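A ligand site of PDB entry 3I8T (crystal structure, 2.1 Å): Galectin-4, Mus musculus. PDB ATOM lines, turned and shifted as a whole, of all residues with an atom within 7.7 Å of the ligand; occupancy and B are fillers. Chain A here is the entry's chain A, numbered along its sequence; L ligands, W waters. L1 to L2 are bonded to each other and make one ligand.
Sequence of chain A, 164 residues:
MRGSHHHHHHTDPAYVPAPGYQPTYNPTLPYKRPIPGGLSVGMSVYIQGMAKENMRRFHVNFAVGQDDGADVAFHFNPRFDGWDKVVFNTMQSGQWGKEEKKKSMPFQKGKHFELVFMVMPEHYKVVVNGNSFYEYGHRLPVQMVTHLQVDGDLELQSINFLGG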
ATOM      1  N   ARG A  57     -29.893  -7.596 -11.606  1.00  0.00           N
ATOM      2  CA  ARG A  57     -29.985  -8.967 -12.100  1.00  0.00           C
ATOM      3  C   ARG A  57     -29.557 -10.029 -11.093  1.00  0.00           C
ATOM      4  O   ARG A  57     -28.970  -9.705 -10.078  1.00  0.00           O
ATOM      5  CB  ARG A  57     -29.243  -9.146 -13.445  1.00  0.00           C
ATOM      6  CG  ARG A  57     -27.852  -8.595 -13.556  1.00  0.00           C
ATOM      7  CD  ARG A  57     -27.261  -8.945 -14.943  1.00  0.00           C
ATOM      8  NE  ARG A  57     -27.367  -7.910 -15.985  1.00  0.00           N
ATOM      9  CZ  ARG A  57     -26.671  -7.921 -17.137  1.00  0.00           C
ATOM     10  NH1 ARG A  57     -26.811  -6.923 -18.017  1.00  0.00           N
ATOM     11  NH2 ARG A  57     -25.807  -8.901 -17.397  1.00  0.00           N
ATOM     12  N   PHE A  58     -29.908 -11.283 -11.363  1.00  0.00           N
ATOM     13  CA  PHE A  58     -29.319 -12.399 -10.630  1.00  0.00           C
ATOM     14  C   PHE A  58     -29.289 -13.600 -11.548  1.00  0.00           C
ATOM     15  O   PHE A  58     -29.882 -13.568 -12.645  1.00  0.00           O
ATOM     16  CB  PHE A  58     -30.018 -12.666  -9.254  1.00  0.00           C
ATOM     17  CG  PHE A  58     -31.448 -13.263  -9.318  1.00  0.00           C
ATOM     18  CD1 PHE A  58     -32.550 -12.449  -9.080  1.00  0.00           C
ATOM     19  CD2 PHE A  58     -31.642 -14.642  -9.495  1.00  0.00           C
ATOM     20  CE1 PHE A  58     -33.858 -12.966  -9.100  1.00  0.00           C
ATOM     21  CE2 PHE A  58     -32.965 -15.202  -9.520  1.00  0.00           C
ATOM     22  CZ  PHE A  58     -34.067 -14.349  -9.303  1.00  0.00           C
ATOM     23  N   HIS A  59     -28.621 -14.660 -11.120  1.00  0.00           N
ATOM     24  CA  HIS A  59     -28.684 -15.865 -11.917  1.00  0.00           C
ATOM     25  C   HIS A  59     -28.735 -17.133 -11.067  1.00  0.00           C
ATOM     26  O   HIS A  59     -28.334 -17.137  -9.900  1.00  0.00           O
ATOM     27  CB  HIS A  59     -27.475 -15.947 -12.903  1.00  0.00           C
ATOM     28  CG  HIS A  59     -26.157 -16.064 -12.221  1.00  0.00           C
ATOM     29  ND1 HIS A  59     -25.400 -14.966 -11.887  1.00  0.00           N
ATOM     30  CD2 HIS A  59     -25.468 -17.145 -11.763  1.00  0.00           C
ATOM     31  CE1 HIS A  59     -24.304 -15.354 -11.263  1.00  0.00           C
ATOM     32  NE2 HIS A  59     -24.316 -16.677 -11.180  1.00  0.00           N
ATOM     33  N   ASN A  61     -27.247 -21.016 -11.884  1.00  0.00           N
ATOM     34  CA  ASN A  61     -26.506 -21.866 -12.792  1.00  0.00           C
ATOM     35  C   ASN A  61     -26.613 -23.330 -12.377  1.00  0.00           C
ATOM     36  O   ASN A  61     -26.399 -23.671 -11.232  1.00  0.00           O
ATOM     37  CB  ASN A  61     -25.025 -21.477 -12.810  1.00  0.00           C
ATOM     38  CG  ASN A  61     -24.787 -20.146 -13.458  1.00  0.00           C
ATOM     39  OD1 ASN A  61     -25.618 -19.680 -14.223  1.00  0.00           O
ATOM     40  ND2 ASN A  61     -23.661 -19.509 -13.131  1.00  0.00           N
ATOM     41  N   HIS A  75     -28.009 -21.587 -17.553  1.00  0.00           N
ATOM     42  CA  HIS A  75     -27.884 -20.298 -16.885  1.00  0.00           C
ATOM     43  C   HIS A  75     -29.240 -19.589 -17.038  1.00  0.00           C
ATOM     44  O   HIS A  75     -29.693 -19.269 -18.164  1.00  0.00           O
ATOM     45  CB  HIS A  75     -26.765 -19.505 -17.620  1.00  0.00           C
ATOM     46  CG  HIS A  75     -26.536 -18.098 -17.118  1.00  0.00           C
ATOM     47  ND1 HIS A  75     -25.962 -17.821 -15.902  1.00  0.00           N
ATOM     48  CD2 HIS A  75     -26.654 -16.904 -17.755  1.00  0.00           C
ATOM     49  CE1 HIS A  75     -25.793 -16.515 -15.770  1.00  0.00           C
ATOM     50  NE2 HIS A  75     -26.229 -15.938 -16.877  1.00  0.00           N
ATOM     51  N   PHE A  76     -29.836 -19.259 -15.894  1.00  0.00           N
ATOM     52  CA  PHE A  76     -31.158 -18.631 -15.842  1.00  0.00           C
ATOM     53  C   PHE A  76     -30.908 -17.236 -15.228  1.00  0.00           C
ATOM     54  O   PHE A  76     -30.431 -17.133 -14.102  1.00  0.00           O
ATOM     55  CB  PHE A  76     -32.093 -19.454 -14.920  1.00  0.00           C
ATOM     56  CG  PHE A  76     -33.425 -18.783 -14.609  1.00  0.00           C
ATOM     57  CD1 PHE A  76     -34.477 -18.875 -15.491  1.00  0.00           C
ATOM     58  CD2 PHE A  76     -33.599 -18.032 -13.426  1.00  0.00           C
ATOM     59  CE1 PHE A  76     -35.715 -18.227 -15.239  1.00  0.00           C
ATOM     60  CE2 PHE A  76     -34.806 -17.414 -13.145  1.00  0.00           C
ATOM     61  CZ  PHE A  76     -35.882 -17.490 -14.043  1.00  0.00           C
ATOM     62  N   ASN A  77     -31.246 -16.169 -15.948  1.00  0.00           N
ATOM     63  CA  ASN A  77     -30.645 -14.865 -15.688  1.00  0.00           C
ATOM     64  C   ASN A  77     -31.636 -13.702 -15.917  1.00  0.00           C
ATOM     65  O   ASN A  77     -31.599 -13.033 -16.962  1.00  0.00           O
ATOM     66  CB  ASN A  77     -29.344 -14.718 -16.527  1.00  0.00           C
ATOM     67  CG  ASN A  77     -28.633 -13.333 -16.365  1.00  0.00           C
ATOM     68  OD1 ASN A  77     -28.097 -12.797 -17.343  1.00  0.00           O
ATOM     69  ND2 ASN A  77     -28.596 -12.801 -15.137  1.00  0.00           N
ATOM     70  N   ARG A  79     -33.018 -10.018 -15.760  1.00  0.00           N
ATOM     71  CA  ARG A  79     -32.327  -8.727 -15.877  1.00  0.00           C
ATOM     72  C   ARG A  79     -33.351  -7.638 -15.996  1.00  0.00           C
ATOM     73  O   ARG A  79     -34.138  -7.665 -16.925  1.00  0.00           O
ATOM     74  CB  ARG A  79     -31.438  -8.662 -17.134  1.00  0.00           C
ATOM     75  CG  ARG A  79     -30.405  -9.785 -17.324  1.00  0.00           C
ATOM     76  CD  ARG A  79     -29.620  -9.554 -18.616  1.00  0.00           C
ATOM     77  NE  ARG A  79     -28.590 -10.571 -18.805  1.00  0.00           N
ATOM     78  CZ  ARG A  79     -27.705 -10.616 -19.807  1.00  0.00           C
ATOM     79  NH1 ARG A  79     -27.674  -9.666 -20.735  1.00  0.00           N
ATOM     80  NH2 ARG A  79     -26.814 -11.624 -19.867  1.00  0.00           N
ATOM     81  N   LYS A  85     -36.349  -8.564 -18.782  1.00  0.00           N
ATOM     82  CA  LYS A  85     -36.354  -9.831 -19.537  1.00  0.00           C
ATOM     83  C   LYS A  85     -35.651 -10.876 -18.690  1.00  0.00           C
ATOM     84  O   LYS A  85     -35.007 -10.535 -17.674  1.00  0.00           O
ATOM     85  CB  LYS A  85     -35.598  -9.698 -20.881  1.00  0.00           C
ATOM     86  CG  LYS A  85     -34.105  -9.342 -20.652  1.00  0.00           C
ATOM     87  CD  LYS A  85     -33.275  -9.337 -21.906  1.00  0.00           C
ATOM     88  CE  LYS A  85     -33.320  -8.027 -22.633  1.00  0.00           C
ATOM     89  NZ  LYS A  85     -32.788  -6.873 -21.852  1.00  0.00           N
ATOM     90  N   VAL A  87     -32.771 -13.919 -19.499  1.00  0.00           N
ATOM     91  CA  VAL A  87     -31.834 -14.454 -20.455  1.00  0.00           C
ATOM     92  C   VAL A  87     -31.537 -15.895 -20.038  1.00  0.00           C
ATOM     93  O   VAL A  87     -31.492 -16.204 -18.848  1.00  0.00           O
ATOM     94  CB  VAL A  87     -30.552 -13.592 -20.517  1.00  0.00           C
ATOM     95  CG1 VAL A  87     -29.394 -14.361 -21.147  1.00  0.00           C
ATOM     96  CG2 VAL A  87     -30.820 -12.316 -21.263  1.00  0.00           C
ATOM     97  N   PHE A  88     -31.419 -16.785 -21.014  1.00  0.00           N
ATOM     98  CA  PHE A  88     -31.118 -18.199 -20.767  1.00  0.00           C
ATOM     99  C   PHE A  88     -29.957 -18.569 -21.667  1.00  0.00           C
ATOM    100  O   PHE A  88     -29.942 -18.200 -22.860  1.00  0.00           O
ATOM    101  CB  PHE A  88     -32.313 -19.104 -21.142  1.00  0.00           C
ATOM    102  CG  PHE A  88     -33.664 -18.603 -20.674  1.00  0.00           C
ATOM    103  CD1 PHE A  88     -34.153 -18.968 -19.417  1.00  0.00           C
ATOM    104  CD2 PHE A  88     -34.439 -17.811 -21.492  1.00  0.00           C
ATOM    105  CE1 PHE A  88     -35.431 -18.545 -18.974  1.00  0.00           C
ATOM    106  CE2 PHE A  88     -35.707 -17.347 -21.030  1.00  0.00           C
ATOM    107  CZ  PHE A  88     -36.165 -17.712 -19.744  1.00  0.00           C
ATOM    108  N   ASN A  89     -28.987 -19.302 -21.120  1.00  0.00           N
ATOM    109  CA  ASN A  89     -27.796 -19.664 -21.938  1.00  0.00           C
ATOM    110  C   ASN A  89     -27.072 -20.883 -21.349  1.00  0.00           C
ATOM    111  O   ASN A  89     -27.489 -21.400 -20.283  1.00  0.00           O
ATOM    112  CB  ASN A  89     -26.831 -18.467 -22.130  1.00  0.00           C
ATOM    113  CG  ASN A  89     -26.116 -18.504 -23.499  1.00  0.00           C
ATOM    114  OD1 ASN A  89     -26.057 -19.550 -24.160  1.00  0.00           O
ATOM    115  ND2 ASN A  89     -25.579 -17.370 -23.915  1.00  0.00           N
ATOM    116  N   THR A  90     -26.034 -21.330 -22.063  1.00  0.00           N
ATOM    117  CA  THR A  90     -25.198 -22.462 -21.690  1.00  0.00           C
ATOM    118  C   THR A  90     -23.785 -21.985 -21.917  1.00  0.00           C
ATOM    119  O   THR A  90     -23.517 -21.327 -22.930  1.00  0.00           O
ATOM    120  CB  THR A  90     -25.521 -23.715 -22.591  1.00  0.00           C
ATOM    121  OG1 THR A  90     -26.823 -24.242 -22.234  1.00  0.00           O
ATOM    122  CG2 THR A  90     -24.465 -24.833 -22.412  1.00  0.00           C
ATOM    123  N   MET A  91     -22.885 -22.286 -20.981  1.00  0.00           N
ATOM    124  CA  MET A  91     -21.464 -22.052 -21.181  1.00  0.00           C
ATOM    125  C   MET A  91     -20.805 -23.419 -21.382  1.00  0.00           C
ATOM    126  O   MET A  91     -20.939 -24.320 -20.530  1.00  0.00           O
ATOM    127  CB  MET A  91     -20.860 -21.375 -19.961  1.00  0.00           C
ATOM    128  CG  MET A  91     -19.322 -21.357 -20.046  1.00  0.00           C
ATOM    129  SD  MET A  91     -18.537 -20.178 -18.924  1.00  0.00           S
ATOM    130  CE  MET A  91     -18.923 -18.686 -19.785  1.00  0.00           C
ATOM    131  N   GLN A  95     -17.286 -21.059 -23.118  1.00  0.00           N
ATOM    132  CA  GLN A  95     -17.877 -20.041 -24.023  1.00  0.00           C
ATOM    133  C   GLN A  95     -19.388 -20.063 -23.925  1.00  0.00           C
ATOM    134  O   GLN A  95     -19.973 -21.144 -24.019  1.00  0.00           O
ATOM    135  CB  GLN A  95     -17.479 -20.302 -25.474  1.00  0.00           C
ATOM    136  CG  GLN A  95     -16.008 -20.057 -25.780  1.00  0.00           C
ATOM    137  CD  GLN A  95     -15.733 -18.634 -26.221  1.00  0.00           C
ATOM    138  OE1 GLN A  95     -15.601 -18.368 -27.413  1.00  0.00           O
ATOM    139  NE2 GLN A  95     -15.644 -17.696 -25.250  1.00  0.00           N
ATOM    140  N   TRP A  96     -20.005 -18.883 -23.767  1.00  0.00           N
ATOM    141  CA  TRP A  96     -21.448 -18.714 -23.818  1.00  0.00           C
ATOM    142  C   TRP A  96     -21.968 -19.023 -25.216  1.00  0.00           C
ATOM    143  O   TRP A  96     -21.366 -18.602 -26.221  1.00  0.00           O
ATOM    144  CB  TRP A  96     -21.848 -17.272 -23.471  1.00  0.00           C
ATOM    145  CG  TRP A  96     -21.653 -16.978 -22.035  1.00  0.00           C
ATOM    146  CD1 TRP A  96     -20.769 -16.097 -21.502  1.00  0.00           C
ATOM    147  CD2 TRP A  96     -22.311 -17.618 -20.915  1.00  0.00           C
ATOM    148  NE1 TRP A  96     -20.851 -16.107 -20.128  1.00  0.00           N
ATOM    149  CE2 TRP A  96     -21.788 -17.021 -19.731  1.00  0.00           C
ATOM    150  CE3 TRP A  96     -23.319 -18.586 -20.805  1.00  0.00           C
ATOM    151  CZ2 TRP A  96     -22.216 -17.386 -18.446  1.00  0.00           C
ATOM    152  CZ3 TRP A  96     -23.764 -18.957 -19.533  1.00  0.00           C
ATOM    153  CH2 TRP A  96     -23.192 -18.361 -18.361  1.00  0.00           C
ATOM    154  N   GLY A  97     -23.094 -19.727 -25.263  1.00  0.00           N
ATOM    155  CA  GLY A  97     -23.714 -20.059 -26.554  1.00  0.00           C
ATOM    156  C   GLY A  97     -24.659 -18.965 -26.996  1.00  0.00           C
ATOM    157  O   GLY A  97     -24.504 -17.799 -26.588  1.00  0.00           O
ATOM    158  N   LYS A  98     -25.623 -19.350 -27.824  1.00  0.00           N
ATOM    159  CA  LYS A  98     -26.654 -18.430 -28.318  1.00  0.00           C
ATOM    160  C   LYS A  98     -27.689 -18.167 -27.231  1.00  0.00           C
ATOM    161  O   LYS A  98     -28.330 -19.097 -26.767  1.00  0.00           O
ATOM    162  CB  LYS A  98     -27.381 -19.020 -29.521  1.00  0.00           C
ATOM    163  CG  LYS A  98     -26.528 -19.202 -30.776  1.00  0.00           C
ATOM    164  CD  LYS A  98     -27.246 -20.208 -31.704  1.00  0.00           C
ATOM    165  CE  LYS A  98     -26.512 -20.438 -33.017  1.00  0.00           C
ATOM    166  NZ  LYS A  98     -27.121 -21.670 -33.685  1.00  0.00           N
ATOM    167  N   GLU A  99     -27.829 -16.917 -26.807  1.00  0.00           N
ATOM    168  CA  GLU A  99     -28.779 -16.568 -25.741  1.00  0.00           C
ATOM    169  C   GLU A  99     -30.162 -16.798 -26.265  1.00  0.00           C
ATOM    170  O   GLU A  99     -30.439 -16.492 -27.424  1.00  0.00           O
ATOM    171  CB  GLU A  99     -28.701 -15.069 -25.368  1.00  0.00           C
ATOM    172  CG  GLU A  99     -27.446 -14.700 -24.697  1.00  0.00           C
ATOM    173  CD  GLU A  99     -27.416 -13.252 -24.169  1.00  0.00           C
ATOM    174  OE1 GLU A  99     -28.243 -12.391 -24.559  1.00  0.00           O
ATOM    175  OE2 GLU A  99     -26.519 -13.004 -23.350  1.00  0.00           O
ATOM    176  N   GLU A 100     -31.002 -17.346 -25.407  1.00  0.00           N
ATOM    177  CA  GLU A 100     -32.428 -17.297 -25.557  1.00  0.00           C
ATOM    178  C   GLU A 100     -32.904 -16.213 -24.605  1.00  0.00           C
ATOM    179  O   GLU A 100     -32.241 -15.913 -23.609  1.00  0.00           O
ATOM    180  CB  GLU A 100     -33.049 -18.683 -25.255  1.00  0.00           C
ATOM    181  CG  GLU A 100     -32.737 -19.726 -26.395  1.00  0.00           C
ATOM    182  CD  GLU A 100     -33.108 -21.164 -26.008  1.00  0.00           C
ATOM    183  OE1 GLU A 100     -34.205 -21.372 -25.429  1.00  0.00           O
ATOM    184  OE2 GLU A 100     -32.311 -22.091 -26.269  1.00  0.00           O
HETATM  185  C1  LIG L   1     -23.280  -9.504 -25.134  1.00  0.00           C
HETATM  186  C2  LIG L   1     -24.627  -9.912 -24.543  1.00  0.00           C
HETATM  187  C3  LIG L   1     -24.557 -10.023 -23.019  1.00  0.00           C
HETATM  188  C4  LIG L   1     -23.410 -10.925 -22.630  1.00  0.00           C
HETATM  189  C5  LIG L   1     -22.078 -10.471 -23.288  1.00  0.00           C
HETATM  190  C6  LIG L   1     -20.907 -11.435 -23.048  1.00  0.00           C
HETATM  191  O1  LIG L   1     -23.003  -8.156 -24.776  1.00  0.00           O
HETATM  192  O2  LIG L   1     -25.573  -8.940 -24.910  1.00  0.00           O
HETATM  193  O3  LIG L   1     -25.791 -10.506 -22.548  1.00  0.00           O
HETATM  194  O4  LIG L   1     -23.330 -10.945 -21.232  1.00  0.00           O
HETATM  195  O5  LIG L   1     -22.245 -10.358 -24.698  1.00  0.00           O
HETATM  196  O6  LIG L   1     -21.140 -12.714 -23.662  1.00  0.00           O
HETATM  197  C1  LG2 L   2     -23.162 -12.179 -20.586  1.00  0.00           C
HETATM  198  C2  LG2 L   2     -22.905 -11.944 -19.091  1.00  0.00           C
HETATM  199  C3  LG2 L   2     -22.891 -13.314 -18.391  1.00  0.00           C
HETATM  200  C4  LG2 L   2     -24.119 -14.132 -18.752  1.00  0.00           C
HETATM  201  C5  LG2 L   2     -24.223 -14.274 -20.268  1.00  0.00           C
HETATM  202  C6  LG2 L   2     -25.388 -15.197 -20.737  1.00  0.00           C
HETATM  203  O1  LG2 L   2     -21.656 -11.282 -18.894  1.00  0.00           O
HETATM  204  O2  LG2 L   2     -22.831 -13.164 -16.994  1.00  0.00           O
HETATM  205  O3  LG2 L   2     -25.303 -13.515 -18.289  1.00  0.00           O
HETATM  206  O4  LG2 L   2     -24.357 -12.968 -20.786  1.00  0.00           O
HETATM  207  O5  LG2 L   2     -25.514 -15.084 -22.138  1.00  0.00           O
HETATM  208  O   HOH W   1     -24.183  -8.549 -19.758  1.00  0.00           O
HETATM  209  O   HOH W   2     -28.146  -9.675 -24.648  1.00  0.00           O
HETATM  210  O   HOH W   3     -23.135 -14.584 -14.698  1.00  0.00           O
HETATM  211  O   HOH W   4     -23.462 -14.211 -24.199  1.00  0.00           O
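Trp 96 touches the ligand.
Within 4 Å of the ligand: His 75, Asn 77, Arg 79, Asn 89, Trp 96 and Glu 99.
The nearest printed residue that does not touch the ligand is Val 87 (4.1 Å).
The guanidinium group of Arg 79 lies within hydrogen-bond range of the side-chain amide oxygen of Asn 77 (2.7 Å).
The backbone NH (N) of Arg 79 is in hydrogen-bond range of the backbone carbonyl oxygen (O) of Lys 85.
N of His 75 is in hydrogen-bond range of O of Asn 89, at 2.8 Å.
The backbone carbonyl oxygen (O) of Gly 97 sits at hydrogen-bond distance from the side-chain amide nitrogen (ND2) of Asn 89 (2.9 Å).
The side-chain amide oxygen (OD1) of Asn 89 lies close to the backbone carbonyl oxygen (O) of Lys 98 (3.5 Å).
OD1 of Asn 61 sits at hydrogen-bond distance from ND1 of His 75 (2.5 Å).
The backbone NH (N) of Asn 77 sits at hydrogen-bond distance from the backbone carbonyl oxygen (O) of Val 87, at 2.9 Å.
The side-chain amide nitrogen (ND2) of Asn 77 lies within hydrogen-bond range of the backbone carbonyl oxygen (O) of Phe 58, at 2.9 Å.
Water W2 bridges an oxygen (O2) of LIG L1 (2.7 Å) and the side-chain carboxylate of Glu 99 (2.7 Å).
Water W4 lies within hydrogen-bond range of O6 of LIG L1 and OE2 of Glu 99.
Water W1 lies within hydrogen-bond range of NH2 of Arg 57 (2.9 Å) and O4 of LIG L1 (2.9 Å).
O5 of LG2 L2 lies within hydrogen-bond range of OE2 of Glu 99, 2.6 Å away.
O3 of LIG L1 is in hydrogen-bond range of NH1 of Arg 79 (2.7 Å).
O5 of LG2 L2 lies within hydrogen-bond range of ND2 of Asn 89.
A ring nitrogen (NE2) of His 75 sits at hydrogen-bond distance from an oxygen (O3) of LG2 L2.
The side-chain amide oxygen (OD1) of Asn 77 lies within hydrogen-bond range of an oxygen (O3) of LG2 L2 (3.0 Å).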
